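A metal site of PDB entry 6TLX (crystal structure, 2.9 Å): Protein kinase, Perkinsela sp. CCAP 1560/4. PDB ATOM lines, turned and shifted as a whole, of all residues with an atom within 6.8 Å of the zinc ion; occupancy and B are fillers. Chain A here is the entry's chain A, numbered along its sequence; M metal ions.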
ATOM      1  N   CYS A  54      12.828   6.561  -3.967  1.00  0.00           N
ATOM      2  CA  CYS A  54      13.461   7.872  -4.169  1.00  0.00           C
ATOM      3  C   CYS A  54      13.562   8.564  -2.800  1.00  0.00           C
ATOM      4  O   CYS A  54      12.588   8.590  -2.054  1.00  0.00           O
ATOM      5  CB  CYS A  54      12.709   8.721  -5.196  1.00  0.00           C
ATOM      6  SG  CYS A  54      13.356  10.411  -5.361  1.00  0.00           S
ATOM      7  N   ASP A  55      14.731   9.078  -2.483  1.00  0.00           N
ATOM      8  CA  ASP A  55      14.862   9.751  -1.186  1.00  0.00           C
ATOM      9  C   ASP A  55      14.134  11.079  -1.254  1.00  0.00           C
ATOM     10  O   ASP A  55      14.137  11.780  -0.271  1.00  0.00           O
ATOM     11  CB  ASP A  55      16.320  10.072  -0.889  1.00  0.00           C
ATOM     12  CG  ASP A  55      17.078   8.917  -0.300  1.00  0.00           C
ATOM     13  OD1 ASP A  55      16.545   7.849  -0.240  1.00  0.00           O
ATOM     14  OD2 ASP A  55      18.200   9.126   0.084  1.00  0.00           O
ATOM     15  N   ARG A  56      13.528  11.421  -2.378  1.00  0.00           N
ATOM     16  CA  ARG A  56      12.889  12.743  -2.381  1.00  0.00           C
ATOM     17  C   ARG A  56      11.402  12.618  -2.610  1.00  0.00           C
ATOM     18  O   ARG A  56      10.684  13.146  -1.835  1.00  0.00           O
ATOM     19  CB  ARG A  56      13.531  13.648  -3.401  1.00  0.00           C
ATOM     20  CG  ARG A  56      12.744  14.927  -3.616  1.00  0.00           C
ATOM     21  CD  ARG A  56      13.564  16.152  -3.926  1.00  0.00           C
ATOM     22  NE  ARG A  56      12.705  17.116  -4.574  1.00  0.00           N
ATOM     23  CZ  ARG A  56      12.082  16.847  -5.693  1.00  0.00           C
ATOM     24  NH1 ARG A  56      11.308  17.754  -6.246  1.00  0.00           N
ATOM     25  NH2 ARG A  56      12.232  15.671  -6.259  1.00  0.00           N
ATOM     26  N   CYS A  57      10.979  11.918  -3.640  1.00  0.00           N
ATOM     27  CA  CYS A  57       9.533  11.845  -3.846  1.00  0.00           C
ATOM     28  C   CYS A  57       9.042  10.511  -3.306  1.00  0.00           C
ATOM     29  O   CYS A  57       7.956  10.170  -3.583  1.00  0.00           O
ATOM     30  CB  CYS A  57       9.222  11.923  -5.319  1.00  0.00           C
ATOM     31  SG  CYS A  57       9.730  10.433  -6.145  1.00  0.00           S
ATOM     32  N   HIS A  58       9.878   9.784  -2.602  1.00  0.00           N
ATOM     33  CA  HIS A  58       9.491   8.521  -1.955  1.00  0.00           C
ATOM     34  C   HIS A  58       8.961   7.458  -2.921  1.00  0.00           C
ATOM     35  O   HIS A  58       8.697   6.349  -2.470  1.00  0.00           O
ATOM     36  CB  HIS A  58       8.530   8.720  -0.779  1.00  0.00           C
ATOM     37  CG  HIS A  58       9.031   9.715   0.210  1.00  0.00           C
ATOM     38  ND1 HIS A  58      10.333   9.671   0.658  1.00  0.00           N
ATOM     39  CD2 HIS A  58       8.405  10.777   0.753  1.00  0.00           C
ATOM     40  CE1 HIS A  58      10.470  10.703   1.486  1.00  0.00           C
ATOM     41  NE2 HIS A  58       9.340  11.411   1.573  1.00  0.00           N
ATOM     42  N   LYS A  59       8.866   7.741  -4.239  1.00  0.00           N
ATOM     43  CA  LYS A  59       8.384   6.729  -5.194  1.00  0.00           C
ATOM     44  C   LYS A  59       9.117   5.414  -5.131  1.00  0.00           C
ATOM     45  O   LYS A  59      10.352   5.397  -5.133  1.00  0.00           O
ATOM     46  CB  LYS A  59       8.379   7.236  -6.653  1.00  0.00           C
ATOM     47  N   VAL A  61      10.453   2.640  -7.021  1.00  0.00           N
ATOM     48  CA  VAL A  61      10.799   2.243  -8.388  1.00  0.00           C
ATOM     49  C   VAL A  61      11.336   0.836  -8.258  1.00  0.00           C
ATOM     50  O   VAL A  61      12.451   0.647  -7.762  1.00  0.00           O
ATOM     51  CB  VAL A  61      11.866   3.162  -9.019  1.00  0.00           C
ATOM     52  CG1 VAL A  61      12.237   2.674 -10.406  1.00  0.00           C
ATOM     53  CG2 VAL A  61      11.411   4.611  -9.055  1.00  0.00           C
ATOM     54  N   ASP A  96      19.324   8.266  -3.196  1.00  0.00           N
ATOM     55  CA  ASP A  96      18.914   7.978  -4.585  1.00  0.00           C
ATOM     56  C   ASP A  96      17.807   8.903  -5.072  1.00  0.00           C
ATOM     57  O   ASP A  96      16.973   9.361  -4.299  1.00  0.00           O
ATOM     58  CB  ASP A  96      18.394   6.555  -4.750  1.00  0.00           C
ATOM     59  CG  ASP A  96      19.394   5.498  -4.381  1.00  0.00           C
ATOM     60  OD1 ASP A  96      20.590   5.736  -4.546  1.00  0.00           O
ATOM     61  OD2 ASP A  96      18.971   4.435  -3.929  1.00  0.00           O
ATOM     62  N   LEU A  97      17.774   9.127  -6.397  1.00  0.00           N
ATOM     63  CA  LEU A  97      16.726   9.921  -7.000  1.00  0.00           C
ATOM     64  C   LEU A  97      16.174   9.198  -8.199  1.00  0.00           C
ATOM     65  O   LEU A  97      16.941   8.744  -9.042  1.00  0.00           O
ATOM     66  CB  LEU A  97      17.259  11.275  -7.418  1.00  0.00           C
ATOM     67  CG  LEU A  97      17.534  12.229  -6.272  1.00  0.00           C
ATOM     68  CD1 LEU A  97      18.422  13.350  -6.708  1.00  0.00           C
ATOM     69  CD2 LEU A  97      16.266  12.747  -5.707  1.00  0.00           C
ATOM     70  N   CYS A  98      14.859   9.098  -8.276  1.00  0.00           N
ATOM     71  CA  CYS A  98      14.158   8.556  -9.434  1.00  0.00           C
ATOM     72  C   CYS A  98      14.387   9.485 -10.651  1.00  0.00           C
ATOM     73  O   CYS A  98      14.769  10.651 -10.485  1.00  0.00           O
ATOM     74  CB  CYS A  98      12.665   8.413  -9.141  1.00  0.00           C
ATOM     75  SG  CYS A  98      11.801   9.996  -8.908  1.00  0.00           S
ATOM     76  N   LYS A  99      14.050   9.030 -11.832  1.00  0.00           N
ATOM     77  CA  LYS A  99      14.290   9.870 -13.021  1.00  0.00           C
ATOM     78  C   LYS A  99      13.487  11.157 -12.929  1.00  0.00           C
ATOM     79  O   LYS A  99      14.011  12.211 -13.180  1.00  0.00           O
ATOM     80  CB  LYS A  99      13.744   9.079 -14.201  1.00  0.00           C
ATOM     81  CG  LYS A  99      14.182   9.545 -15.569  1.00  0.00           C
ATOM     82  CD  LYS A  99      13.814   8.531 -16.598  1.00  0.00           C
ATOM     83  CE  LYS A  99      13.710   9.077 -17.998  1.00  0.00           C
ATOM     84  NZ  LYS A  99      12.998   8.106 -18.853  1.00  0.00           N
ATOM     85  N   ALA A 100      12.255  11.026 -12.491  1.00  0.00           N
ATOM     86  CA  ALA A 100      11.351  12.163 -12.400  1.00  0.00           C
ATOM     87  C   ALA A 100      11.936  13.299 -11.597  1.00  0.00           C
ATOM     88  O   ALA A 100      11.860  14.449 -12.026  1.00  0.00           O
ATOM     89  CB  ALA A 100      10.023  11.732 -11.818  1.00  0.00           C
ATOM     90  N   CYS A 101      12.542  12.995 -10.440  1.00  0.00           N
ATOM     91  CA  CYS A 101      13.159  14.007  -9.572  1.00  0.00           C
ATOM     92  C   CYS A 101      14.394  14.612 -10.252  1.00  0.00           C
ATOM     93  O   CYS A 101      14.640  15.805 -10.145  1.00  0.00           O
ATOM     94  CB  CYS A 101      13.495  13.415  -8.206  1.00  0.00           C
ATOM     95  SG  CYS A 101      12.075  13.186  -7.105  1.00  0.00           S
ATOM     96  N   GLY A 102      15.140  13.793 -10.974  1.00  0.00           N
ATOM     97  CA  GLY A 102      16.300  14.258 -11.723  1.00  0.00           C
ATOM     98  C   GLY A 102      15.848  15.220 -12.808  1.00  0.00           C
ATOM     99  O   GLY A 102      16.372  16.327 -12.937  1.00  0.00           O
HETATM  100 ZN    ZN M   1      11.604  11.022  -7.012  1.00  0.00          ZN
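Within 4 Å of the zinc ion: Cys 54, Cys 57, Cys 98 and Cys 101. The nearest printed residue that does not touch the zinc ion is Arg 56 (4.7 Å).
The side-chain sulfur (SG) of Cys 57 lies close to the backbone NH (N) of Lys 59, 3.4 Å away. SG of Cys 98 lies close to N of Ala 100 (3.8 Å). The side-chain sulfur of Cys 101 lies close to the guanidinium group of Arg 56. The side-chain sulfur of Cys 54 sits close to the backbone NH of Arg 56 (3.2 Å). N of Cys 54 is in hydrogen-bond range of O of Lys 59 (3.0 Å).
The zinc ion is bound by SG of Cys 57 (2.1 Å), SG of Cys 98 (2.2 Å), SG of Cys 101 (2.2 Å) and SG of Cys 54 (2.5 Å). The zinc ion has four donor atoms within binding distance.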
